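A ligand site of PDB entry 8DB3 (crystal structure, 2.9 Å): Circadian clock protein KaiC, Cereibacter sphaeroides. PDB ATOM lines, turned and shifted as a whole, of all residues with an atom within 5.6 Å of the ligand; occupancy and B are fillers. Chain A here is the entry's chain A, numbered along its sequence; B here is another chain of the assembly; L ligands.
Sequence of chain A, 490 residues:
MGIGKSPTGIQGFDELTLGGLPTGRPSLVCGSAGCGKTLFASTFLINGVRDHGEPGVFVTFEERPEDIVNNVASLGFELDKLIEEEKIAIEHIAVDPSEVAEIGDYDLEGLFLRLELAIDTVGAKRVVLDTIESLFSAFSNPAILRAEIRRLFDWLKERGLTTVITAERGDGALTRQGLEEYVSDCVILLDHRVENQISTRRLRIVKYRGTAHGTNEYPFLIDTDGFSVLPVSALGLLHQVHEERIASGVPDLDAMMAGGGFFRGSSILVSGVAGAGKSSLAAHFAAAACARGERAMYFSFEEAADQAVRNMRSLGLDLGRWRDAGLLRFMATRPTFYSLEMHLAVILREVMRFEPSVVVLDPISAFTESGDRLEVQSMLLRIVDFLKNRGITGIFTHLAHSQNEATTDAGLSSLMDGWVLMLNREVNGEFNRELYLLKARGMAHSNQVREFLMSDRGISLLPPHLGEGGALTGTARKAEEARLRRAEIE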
ATOM      1  N   GLY A  31      13.331  15.538  28.209  1.00  0.00           N
ATOM      2  CA  GLY A  31      14.521  15.220  27.453  1.00  0.00           C
ATOM      3  C   GLY A  31      14.554  15.903  26.098  1.00  0.00           C
ATOM      4  O   GLY A  31      13.512  16.340  25.594  1.00  0.00           O
ATOM      5  N   SER A  32      15.737  16.028  25.519  1.00  0.00           N
ATOM      6  CA  SER A  32      15.858  16.513  24.158  1.00  0.00           C
ATOM      7  C   SER A  32      15.402  15.434  23.190  1.00  0.00           C
ATOM      8  O   SER A  32      14.956  14.347  23.577  1.00  0.00           O
ATOM      9  CB  SER A  32      17.291  16.950  23.880  1.00  0.00           C
ATOM     10  OG  SER A  32      18.221  16.093  24.518  1.00  0.00           O
ATOM     11  N   ALA A  33      15.496  15.726  21.892  1.00  0.00           N
ATOM     12  CA  ALA A  33      15.016  14.802  20.873  1.00  0.00           C
ATOM     13  C   ALA A  33      15.860  13.533  20.872  1.00  0.00           C
ATOM     14  O   ALA A  33      17.089  13.580  20.850  1.00  0.00           O
ATOM     15  CB  ALA A  33      15.057  15.466  19.494  1.00  0.00           C
ATOM     16  N   GLY A  34      15.183  12.388  20.919  1.00  0.00           N
ATOM     17  CA  GLY A  34      15.868  11.112  20.835  1.00  0.00           C
ATOM     18  C   GLY A  34      16.455  10.603  22.123  1.00  0.00           C
ATOM     19  O   GLY A  34      17.411   9.830  22.095  1.00  0.00           O
ATOM     20  N   CYS A  35      15.900  11.014  23.270  1.00  0.00           N
ATOM     21  CA  CYS A  35      16.453  10.630  24.558  1.00  0.00           C
ATOM     22  C   CYS A  35      15.749   9.441  25.192  1.00  0.00           C
ATOM     23  O   CYS A  35      16.341   8.784  26.058  1.00  0.00           O
ATOM     24  CB  CYS A  35      16.400  11.824  25.520  1.00  0.00           C
ATOM     25  SG  CYS A  35      17.631  13.090  25.128  1.00  0.00           S
ATOM     26  N   GLY A  36      14.512   9.153  24.810  1.00  0.00           N
ATOM     27  CA  GLY A  36      13.825   7.969  25.280  1.00  0.00           C
ATOM     28  C   GLY A  36      12.580   8.224  26.096  1.00  0.00           C
ATOM     29  O   GLY A  36      12.072   7.314  26.753  1.00  0.00           O
ATOM     30  N   LYS A  37      12.054   9.462  26.061  1.00  0.00           N
ATOM     31  CA  LYS A  37      10.879   9.765  26.859  1.00  0.00           C
ATOM     32  C   LYS A  37       9.633   9.054  26.312  1.00  0.00           C
ATOM     33  O   LYS A  37       8.836   8.505  27.084  1.00  0.00           O
ATOM     34  CB  LYS A  37      10.645  11.279  26.926  1.00  0.00           C
ATOM     35  CG  LYS A  37      11.041  12.057  25.670  1.00  0.00           C
ATOM     36  CD  LYS A  37      10.828  13.557  25.836  1.00  0.00           C
ATOM     37  CE  LYS A  37      11.190  14.304  24.553  1.00  0.00           C
ATOM     38  NZ  LYS A  37      10.070  14.299  23.564  1.00  0.00           N
ATOM     39  N   THR A  38       9.476   9.054  24.988  1.00  0.00           N
ATOM     40  CA  THR A  38       8.319   8.386  24.392  1.00  0.00           C
ATOM     41  C   THR A  38       8.364   6.882  24.645  1.00  0.00           C
ATOM     42  O   THR A  38       7.357   6.275  25.008  1.00  0.00           O
ATOM     43  CB  THR A  38       8.277   8.665  22.887  1.00  0.00           C
ATOM     44  OG1 THR A  38       8.155  10.069  22.646  1.00  0.00           O
ATOM     45  CG2 THR A  38       7.079   7.950  22.250  1.00  0.00           C
ATOM     46  N   LEU A  39       9.528   6.265  24.445  1.00  0.00           N
ATOM     47  CA  LEU A  39       9.650   4.840  24.721  1.00  0.00           C
ATOM     48  C   LEU A  39       9.439   4.550  26.204  1.00  0.00           C
ATOM     49  O   LEU A  39       8.844   3.522  26.562  1.00  0.00           O
ATOM     50  CB  LEU A  39      11.008   4.317  24.269  1.00  0.00           C
ATOM     51  CG  LEU A  39      11.290   2.848  24.565  1.00  0.00           C
ATOM     52  CD1 LEU A  39      10.887   1.971  23.392  1.00  0.00           C
ATOM     53  CD2 LEU A  39      12.765   2.638  24.887  1.00  0.00           C
ATOM     54  N   PHE A  40       9.930   5.435  27.073  1.00  0.00           N
ATOM     55  CA  PHE A  40       9.695   5.259  28.505  1.00  0.00           C
ATOM     56  C   PHE A  40       8.204   5.241  28.803  1.00  0.00           C
ATOM     57  O   PHE A  40       7.712   4.386  29.555  1.00  0.00           O
ATOM     58  CB  PHE A  40      10.398   6.368  29.278  1.00  0.00           C
ATOM     59  CG  PHE A  40      10.147   6.336  30.768  1.00  0.00           C
ATOM     60  CD1 PHE A  40      10.959   5.586  31.601  1.00  0.00           C
ATOM     61  CD2 PHE A  40       9.101   7.052  31.322  1.00  0.00           C
ATOM     62  CE1 PHE A  40      10.737   5.556  32.963  1.00  0.00           C
ATOM     63  CE2 PHE A  40       8.870   7.026  32.682  1.00  0.00           C
ATOM     64  CZ  PHE A  40       9.688   6.278  33.502  1.00  0.00           C
ATOM     65  N   ASN A  71       6.630   2.107  15.657  1.00  0.00           N
ATOM     66  CA  ASN A  71       7.897   2.502  16.265  1.00  0.00           C
ATOM     67  C   ASN A  71       8.264   1.643  17.468  1.00  0.00           C
ATOM     68  O   ASN A  71       9.376   1.768  17.978  1.00  0.00           O
ATOM     69  CB  ASN A  71       7.832   3.976  16.682  1.00  0.00           C
ATOM     70  CG  ASN A  71       7.785   4.916  15.496  1.00  0.00           C
ATOM     71  OD1 ASN A  71       7.980   4.505  14.346  1.00  0.00           O
ATOM     72  ND2 ASN A  71       7.526   6.191  15.765  1.00  0.00           N
ATOM     73  N   VAL A  72       7.357   0.781  17.912  1.00  0.00           N
ATOM     74  CA  VAL A  72       7.628  -0.123  19.028  1.00  0.00           C
ATOM     75  C   VAL A  72       7.400  -1.580  18.655  1.00  0.00           C
ATOM     76  O   VAL A  72       7.746  -2.469  19.439  1.00  0.00           O
ATOM     77  CB  VAL A  72       6.793   0.249  20.261  1.00  0.00           C
ATOM     78  CG1 VAL A  72       5.360  -0.257  20.131  1.00  0.00           C
ATOM     79  CG2 VAL A  72       7.433  -0.285  21.527  1.00  0.00           C
ATOM     80  N   SER A  74       9.118  -3.305  16.700  1.00  0.00           N
ATOM     81  CA  SER A  74      10.414  -3.977  16.630  1.00  0.00           C
ATOM     82  C   SER A  74      10.824  -4.544  17.989  1.00  0.00           C
ATOM     83  O   SER A  74      11.506  -5.572  18.041  1.00  0.00           O
ATOM     84  CB  SER A  74      11.483  -3.002  16.118  1.00  0.00           C
ATOM     85  OG  SER A  74      12.720  -3.184  16.796  1.00  0.00           O
ATOM     86  N   LEU A  75      10.413  -3.905  19.074  1.00  0.00           N
ATOM     87  CA  LEU A  75      10.758  -4.344  20.421  1.00  0.00           C
ATOM     88  C   LEU A  75       9.894  -5.492  20.910  1.00  0.00           C
ATOM     89  O   LEU A  75       9.993  -5.865  22.088  1.00  0.00           O
ATOM     90  CB  LEU A  75      10.661  -3.176  21.399  1.00  0.00           C
ATOM     91  CG  LEU A  75      11.552  -1.980  21.031  1.00  0.00           C
ATOM     92  CD1 LEU A  75      10.950  -0.684  21.549  1.00  0.00           C
ATOM     93  CD2 LEU A  75      12.959  -2.182  21.590  1.00  0.00           C
ATOM     94  N   ASP A 130       1.588  12.607  25.240  1.00  0.00           N
ATOM     95  CA  ASP A 130       2.746  12.831  24.389  1.00  0.00           C
ATOM     96  C   ASP A 130       2.496  14.075  23.553  1.00  0.00           C
ATOM     97  O   ASP A 130       1.514  14.144  22.806  1.00  0.00           O
ATOM     98  CB  ASP A 130       3.010  11.625  23.497  1.00  0.00           C
ATOM     99  CG  ASP A 130       4.480  11.485  23.115  1.00  0.00           C
ATOM    100  OD1 ASP A 130       5.335  12.107  23.778  1.00  0.00           O
ATOM    101  OD2 ASP A 130       4.776  10.756  22.151  1.00  0.00           O
ATOM    102  N   ARG A 201      23.491   7.297  27.479  1.00  0.00           N
ATOM    103  CA  ARG A 201      22.150   7.691  27.899  1.00  0.00           C
ATOM    104  C   ARG A 201      22.077   7.652  29.423  1.00  0.00           C
ATOM    105  O   ARG A 201      22.376   6.613  30.028  1.00  0.00           O
ATOM    106  CB  ARG A 201      21.084   6.777  27.312  1.00  0.00           C
ATOM    107  CG  ARG A 201      21.480   6.090  26.025  1.00  0.00           C
ATOM    108  CD  ARG A 201      20.275   5.442  25.351  1.00  0.00           C
ATOM    109  NE  ARG A 201      19.487   6.425  24.616  1.00  0.00           N
ATOM    110  CZ  ARG A 201      19.098   6.290  23.350  1.00  0.00           C
ATOM    111  NH1 ARG A 201      19.387   5.205  22.654  1.00  0.00           N
ATOM    112  NH2 ARG A 201      18.422   7.281  22.780  1.00  0.00           N
ATOM    113  N   ILE A 222      18.685   1.813  25.602  1.00  0.00           N
ATOM    114  CA  ILE A 222      17.508   1.521  24.786  1.00  0.00           C
ATOM    115  C   ILE A 222      17.936   0.491  23.746  1.00  0.00           C
ATOM    116  O   ILE A 222      18.233   0.836  22.596  1.00  0.00           O
ATOM    117  CB  ILE A 222      16.922   2.783  24.132  1.00  0.00           C
ATOM    118  CG1 ILE A 222      16.550   3.804  25.209  1.00  0.00           C
ATOM    119  CG2 ILE A 222      15.708   2.404  23.308  1.00  0.00           C
ATOM    120  CD1 ILE A 222      15.914   5.062  24.673  1.00  0.00           C
ATOM    121  N   ASP A 223      17.968  -0.774  24.153  1.00  0.00           N
ATOM    122  CA  ASP A 223      18.395  -1.833  23.255  1.00  0.00           C
ATOM    123  C   ASP A 223      17.174  -2.381  22.514  1.00  0.00           C
ATOM    124  O   ASP A 223      16.066  -1.857  22.627  1.00  0.00           O
ATOM    125  CB  ASP A 223      19.132  -2.922  24.027  1.00  0.00           C
ATOM    126  CG  ASP A 223      18.289  -3.530  25.142  1.00  0.00           C
ATOM    127  OD1 ASP A 223      17.130  -3.103  25.310  1.00  0.00           O
ATOM    128  OD2 ASP A 223      18.800  -4.427  25.846  1.00  0.00           O
ATOM    129  N   THR A 224      17.365  -3.448  21.741  1.00  0.00           N
ATOM    130  CA  THR A 224      16.232  -4.092  21.074  1.00  0.00           C
ATOM    131  C   THR A 224      15.262  -4.711  22.072  1.00  0.00           C
ATOM    132  O   THR A 224      14.133  -5.032  21.706  1.00  0.00           O
ATOM    133  CB  THR A 224      16.730  -5.154  20.096  1.00  0.00           C
ATOM    134  OG1 THR A 224      17.481  -6.151  20.805  1.00  0.00           O
ATOM    135  CG2 THR A 224      17.610  -4.522  19.024  1.00  0.00           C
ATOM    136  N   TYR B 182      11.865  17.572  16.739  1.00  0.00           N
ATOM    137  CA  TYR B 182      10.888  16.868  17.556  1.00  0.00           C
ATOM    138  C   TYR B 182       9.719  16.348  16.741  1.00  0.00           C
ATOM    139  O   TYR B 182       9.107  15.334  17.103  1.00  0.00           O
ATOM    140  CB  TYR B 182      10.373  17.775  18.677  1.00  0.00           C
ATOM    141  CG  TYR B 182      11.449  18.186  19.659  1.00  0.00           C
ATOM    142  CD1 TYR B 182      11.774  17.380  20.752  1.00  0.00           C
ATOM    143  CD2 TYR B 182      12.150  19.371  19.497  1.00  0.00           C
ATOM    144  CE1 TYR B 182      12.759  17.753  21.643  1.00  0.00           C
ATOM    145  CE2 TYR B 182      13.141  19.751  20.383  1.00  0.00           C
ATOM    146  CZ  TYR B 182      13.443  18.933  21.449  1.00  0.00           C
ATOM    147  OH  TYR B 182      14.425  19.318  22.333  1.00  0.00           O
ATOM    148  N   VAL B 206      20.667  11.509  15.997  1.00  0.00           N
ATOM    149  CA  VAL B 206      20.118  12.043  17.247  1.00  0.00           C
ATOM    150  C   VAL B 206      18.848  11.289  17.629  1.00  0.00           C
ATOM    151  O   VAL B 206      18.616  11.009  18.810  1.00  0.00           O
ATOM    152  CB  VAL B 206      19.861  13.555  17.109  1.00  0.00           C
ATOM    153  CG1 VAL B 206      19.255  14.108  18.385  1.00  0.00           C
ATOM    154  CG2 VAL B 206      21.145  14.285  16.751  1.00  0.00           C
ATOM    155  N   LYS B 207      18.020  10.950  16.647  1.00  0.00           N
ATOM    156  CA  LYS B 207      16.779  10.239  16.902  1.00  0.00           C
ATOM    157  C   LYS B 207      16.458   9.366  15.702  1.00  0.00           C
ATOM    158  O   LYS B 207      16.706   9.755  14.563  1.00  0.00           O
ATOM    159  CB  LYS B 207      15.624  11.213  17.178  1.00  0.00           C
ATOM    160  CG  LYS B 207      14.340  10.539  17.608  1.00  0.00           C
ATOM    161  CD  LYS B 207      13.118  11.255  17.056  1.00  0.00           C
ATOM    162  CE  LYS B 207      13.042  12.686  17.577  1.00  0.00           C
ATOM    163  NZ  LYS B 207      11.670  13.242  17.438  1.00  0.00           N
ATOM    164  N   TYR B 208      15.915   8.179  15.976  1.00  0.00           N
ATOM    165  CA  TYR B 208      15.471   7.271  14.912  1.00  0.00           C
ATOM    166  C   TYR B 208      14.462   6.325  15.556  1.00  0.00           C
ATOM    167  O   TYR B 208      14.827   5.285  16.103  1.00  0.00           O
ATOM    168  CB  TYR B 208      16.628   6.528  14.290  1.00  0.00           C
ATOM    169  CG  TYR B 208      16.334   5.887  12.949  1.00  0.00           C
ATOM    170  CD1 TYR B 208      15.023   5.648  12.553  1.00  0.00           C
ATOM    171  CD2 TYR B 208      17.357   5.508  12.104  1.00  0.00           C
ATOM    172  CE1 TYR B 208      14.747   5.061  11.329  1.00  0.00           C
ATOM    173  CE2 TYR B 208      17.096   4.923  10.879  1.00  0.00           C
ATOM    174  CZ  TYR B 208      15.785   4.694  10.501  1.00  0.00           C
ATOM    175  OH  TYR B 208      15.518   4.106   9.289  1.00  0.00           O
ATOM    176  N   ARG B 209      13.191   6.695  15.472  1.00  0.00           N
ATOM    177  CA  ARG B 209      12.134   5.892  16.082  1.00  0.00           C
ATOM    178  C   ARG B 209      11.891   4.626  15.271  1.00  0.00           C
ATOM    179  O   ARG B 209      11.811   4.661  14.040  1.00  0.00           O
ATOM    180  CB  ARG B 209      10.856   6.715  16.194  1.00  0.00           C
ATOM    181  CG  ARG B 209      10.964   7.816  17.238  1.00  0.00           C
ATOM    182  CD  ARG B 209       9.777   8.758  17.246  1.00  0.00           C
ATOM    183  NE  ARG B 209       9.742   9.508  18.500  1.00  0.00           N
ATOM    184  CZ  ARG B 209       8.814  10.398  18.817  1.00  0.00           C
ATOM    185  NH1 ARG B 209       7.840  10.719  17.987  1.00  0.00           N
ATOM    186  NH2 ARG B 209       8.864  10.980  20.015  1.00  0.00           N
ATOM    187  N   GLY B 210      11.778   3.496  15.983  1.00  0.00           N
ATOM    188  CA  GLY B 210      11.405   2.239  15.376  1.00  0.00           C
ATOM    189  C   GLY B 210      12.532   1.266  15.112  1.00  0.00           C
ATOM    190  O   GLY B 210      12.277   0.182  14.577  1.00  0.00           O
ATOM    191  N   THR B 211      13.764   1.615  15.471  1.00  0.00           N
ATOM    192  CA  THR B 211      14.886   0.744  15.185  1.00  0.00           C
ATOM    193  C   THR B 211      16.051   1.055  16.116  1.00  0.00           C
ATOM    194  O   THR B 211      16.146   2.156  16.657  1.00  0.00           O
ATOM    195  CB  THR B 211      15.356   0.874  13.727  1.00  0.00           C
ATOM    196  OG1 THR B 211      16.550   0.109  13.528  1.00  0.00           O
ATOM    197  CG2 THR B 211      15.644   2.349  13.390  1.00  0.00           C
ATOM    198  N   ALA B 212      16.933   0.072  16.276  1.00  0.00           N
ATOM    199  CA  ALA B 212      18.241   0.323  16.860  1.00  0.00           C
ATOM    200  C   ALA B 212      19.152   0.953  15.800  1.00  0.00           C
ATOM    201  O   ALA B 212      18.884   0.869  14.593  1.00  0.00           O
ATOM    202  CB  ALA B 212      18.846  -0.968  17.392  1.00  0.00           C
ATOM    203  N   HIS B 213      20.212   1.593  16.265  1.00  0.00           N
ATOM    204  CA  HIS B 213      21.113   2.307  15.364  1.00  0.00           C
ATOM    205  C   HIS B 213      22.325   2.793  16.128  1.00  0.00           C
ATOM    206  O   HIS B 213      22.388   2.685  17.355  1.00  0.00           O
ATOM    207  CB  HIS B 213      20.390   3.479  14.706  1.00  0.00           C
ATOM    208  CG  HIS B 213      19.897   4.507  15.679  1.00  0.00           C
ATOM    209  ND1 HIS B 213      20.668   5.568  16.100  1.00  0.00           N
ATOM    210  CD2 HIS B 213      18.722   4.616  16.335  1.00  0.00           C
ATOM    211  CE1 HIS B 213      19.986   6.301  16.957  1.00  0.00           C
ATOM    212  NE2 HIS B 213      18.804   5.744  17.124  1.00  0.00           N
ATOM    213  N   THR B 215      24.386   5.230  17.972  1.00  0.00           N
ATOM    214  CA  THR B 215      24.178   6.443  18.733  1.00  0.00           C
ATOM    215  C   THR B 215      25.427   7.307  18.828  1.00  0.00           C
ATOM    216  O   THR B 215      25.320   8.479  19.219  1.00  0.00           O
ATOM    217  CB  THR B 215      23.702   6.098  20.150  1.00  0.00           C
ATOM    218  OG1 THR B 215      24.447   4.980  20.640  1.00  0.00           O
ATOM    219  CG2 THR B 215      22.220   5.754  20.137  1.00  0.00           C
HETATM  220  P1  LIG L   1      11.807  10.993  22.225  1.00  0.00           P
HETATM  221  O1  LIG L   1      11.588  11.982  21.108  1.00  0.00           O
HETATM  222  O2  LIG L   1      12.859  11.392  23.225  1.00  0.00           O
HETATM  223  O3  LIG L   1      10.534  10.490  22.869  1.00  0.00           O
HETATM  224  P2  LIG L   1      11.734   8.255  21.600  1.00  0.00           P
HETATM  225  O4  LIG L   1      10.662   8.177  20.548  1.00  0.00           O
HETATM  226  O5  LIG L   1      11.396   8.020  23.056  1.00  0.00           O
HETATM  227  O6  LIG L   1      12.428   9.697  21.489  1.00  0.00           O
HETATM  228  O7  LIG L   1      12.925   7.246  21.217  1.00  0.00           O
HETATM  229  C1  LIG L   1      14.248   7.674  21.473  1.00  0.00           C
HETATM  230  C2  LIG L   1      15.251   6.598  21.177  1.00  0.00           C
HETATM  231  O8  LIG L   1      14.682   5.278  21.354  1.00  0.00           O
HETATM  232  C3  LIG L   1      15.825   6.635  19.746  1.00  0.00           C
HETATM  233  O9  LIG L   1      16.990   7.423  19.691  1.00  0.00           O
HETATM  234  C4  LIG L   1      16.111   5.163  19.437  1.00  0.00           C
HETATM  235  O10 LIG L   1      17.499   4.868  19.567  1.00  0.00           O
HETATM  236  C5  LIG L   1      15.361   4.344  20.507  1.00  0.00           C
HETATM  237  N1  LIG L   1      14.406   3.411  19.916  1.00  0.00           N
HETATM  238  C6  LIG L   1      13.147   3.703  19.521  1.00  0.00           C
HETATM  239  N2  LIG L   1      12.526   2.601  19.040  1.00  0.00           N
HETATM  240  C7  LIG L   1      13.403   1.591  19.123  1.00  0.00           C
HETATM  241  C8  LIG L   1      13.384   0.154  18.778  1.00  0.00           C
HETATM  242  N3  LIG L   1      12.286  -0.388  18.237  1.00  0.00           N
HETATM  243  N4  LIG L   1      14.501  -0.570  19.029  1.00  0.00           N
HETATM  244  C9  LIG L   1      15.605  -0.020  19.566  1.00  0.00           C
HETATM  245  N5  LIG L   1      15.680   1.284  19.902  1.00  0.00           N
HETATM  246  C10 LIG L   1      14.633   2.112  19.707  1.00  0.00           C
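N of Thr 38 lies within hydrogen-bond range of O3 of the ligand (2.8 Å).
An oxygen (O3) of the ligand lies within hydrogen-bond range of the side-chain hydroxyl (OG1) of Thr 38 (2.4 Å).
NE of Arg 209 of chain B lies within salt-bridge range of O4 of the ligand, 2.6 Å away.
NE2 of His 213 of chain B is in hydrogen-bond range of O10 of the ligand.
The backbone NH of Leu 39 sits at hydrogen-bond distance from an oxygen (O5) of the ligand.
An oxygen (O2) of the ligand lies within hydrogen-bond range of the backbone NH of Cys 35, at 3.1 Å.
An oxygen (O5) of the ligand is in hydrogen-bond range of the backbone NH (N) of Lys 37 (3.4 Å).
The side-chain amino group of Lys 37 is in salt-bridge range of an oxygen (O1) of the ligand.
OG of Ser 74 sits at hydrogen-bond distance from N3 of the ligand (3.2 Å).
The backbone NH (N) of Gly 36 is in hydrogen-bond range of an oxygen (O2) of the ligand, 3.2 Å away.
N of Gly 210 of chain B sits at hydrogen-bond distance from N2 of the ligand, at 3.3 Å.
O9 of the ligand lies within hydrogen-bond range of NH2 of Arg 201, at 3.4 Å.
The backbone NH (N) of Gly 34 lies within hydrogen-bond range of an oxygen (O2) of the ligand (3.4 Å).
The backbone carbonyl oxygen (O) of Gly 34 is in hydrogen-bond range of an oxygen (O9) of the ligand.
The side-chain amino group of Lys 207 of chain B is in salt-bridge range of an oxygen (O1) of the ligand (3.9 Å).
The side-chain hydroxyl (OG1) of Thr 38 is in hydrogen-bond range of the guanidinium group (NH2) of Arg 209 of chain B.
The side-chain carboxylate (OD2) of Asp 130 lies within hydrogen-bond range of the side-chain hydroxyl (OG1) of Thr 38, at 3.5 Å.
SG of Cys 35 sits at hydrogen-bond distance from OG of Ser 32 (3.1 Å).
The guanidinium group of Arg 201 is in hydrogen-bond range of the backbone carbonyl oxygen of Gly 34 (2.8 Å).
NZ of Lys 207 of chain B is in hydrogen-bond range of O of Tyr 182 of chain B, at 3.3 Å.
N2 of the ligand sits close to O of Asn 71, 3.4 Å away.
O of Thr 211 of chain B sits close to N5 of the ligand (3.4 Å).
Ser 32 touches the ligand.
CG of Leu 75 touches N3 of the ligand (3.3 Å).
Ile 222 touches the ligand.
O of Asp 223 touches C9 of the ligand (3.6 Å).
Tyr 208 of chain B touches the ligand.
N of Ala 212 of chain B touches C9 of the ligand, at 3.5 Å.
Hydrophobic or aromatic side chains within 4 Å of the ligand: Leu 39, Leu 75, Ile 222 and His 213 of chain B.
Of the 29 residues printed, 20 come within 4 Å of the ligand.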
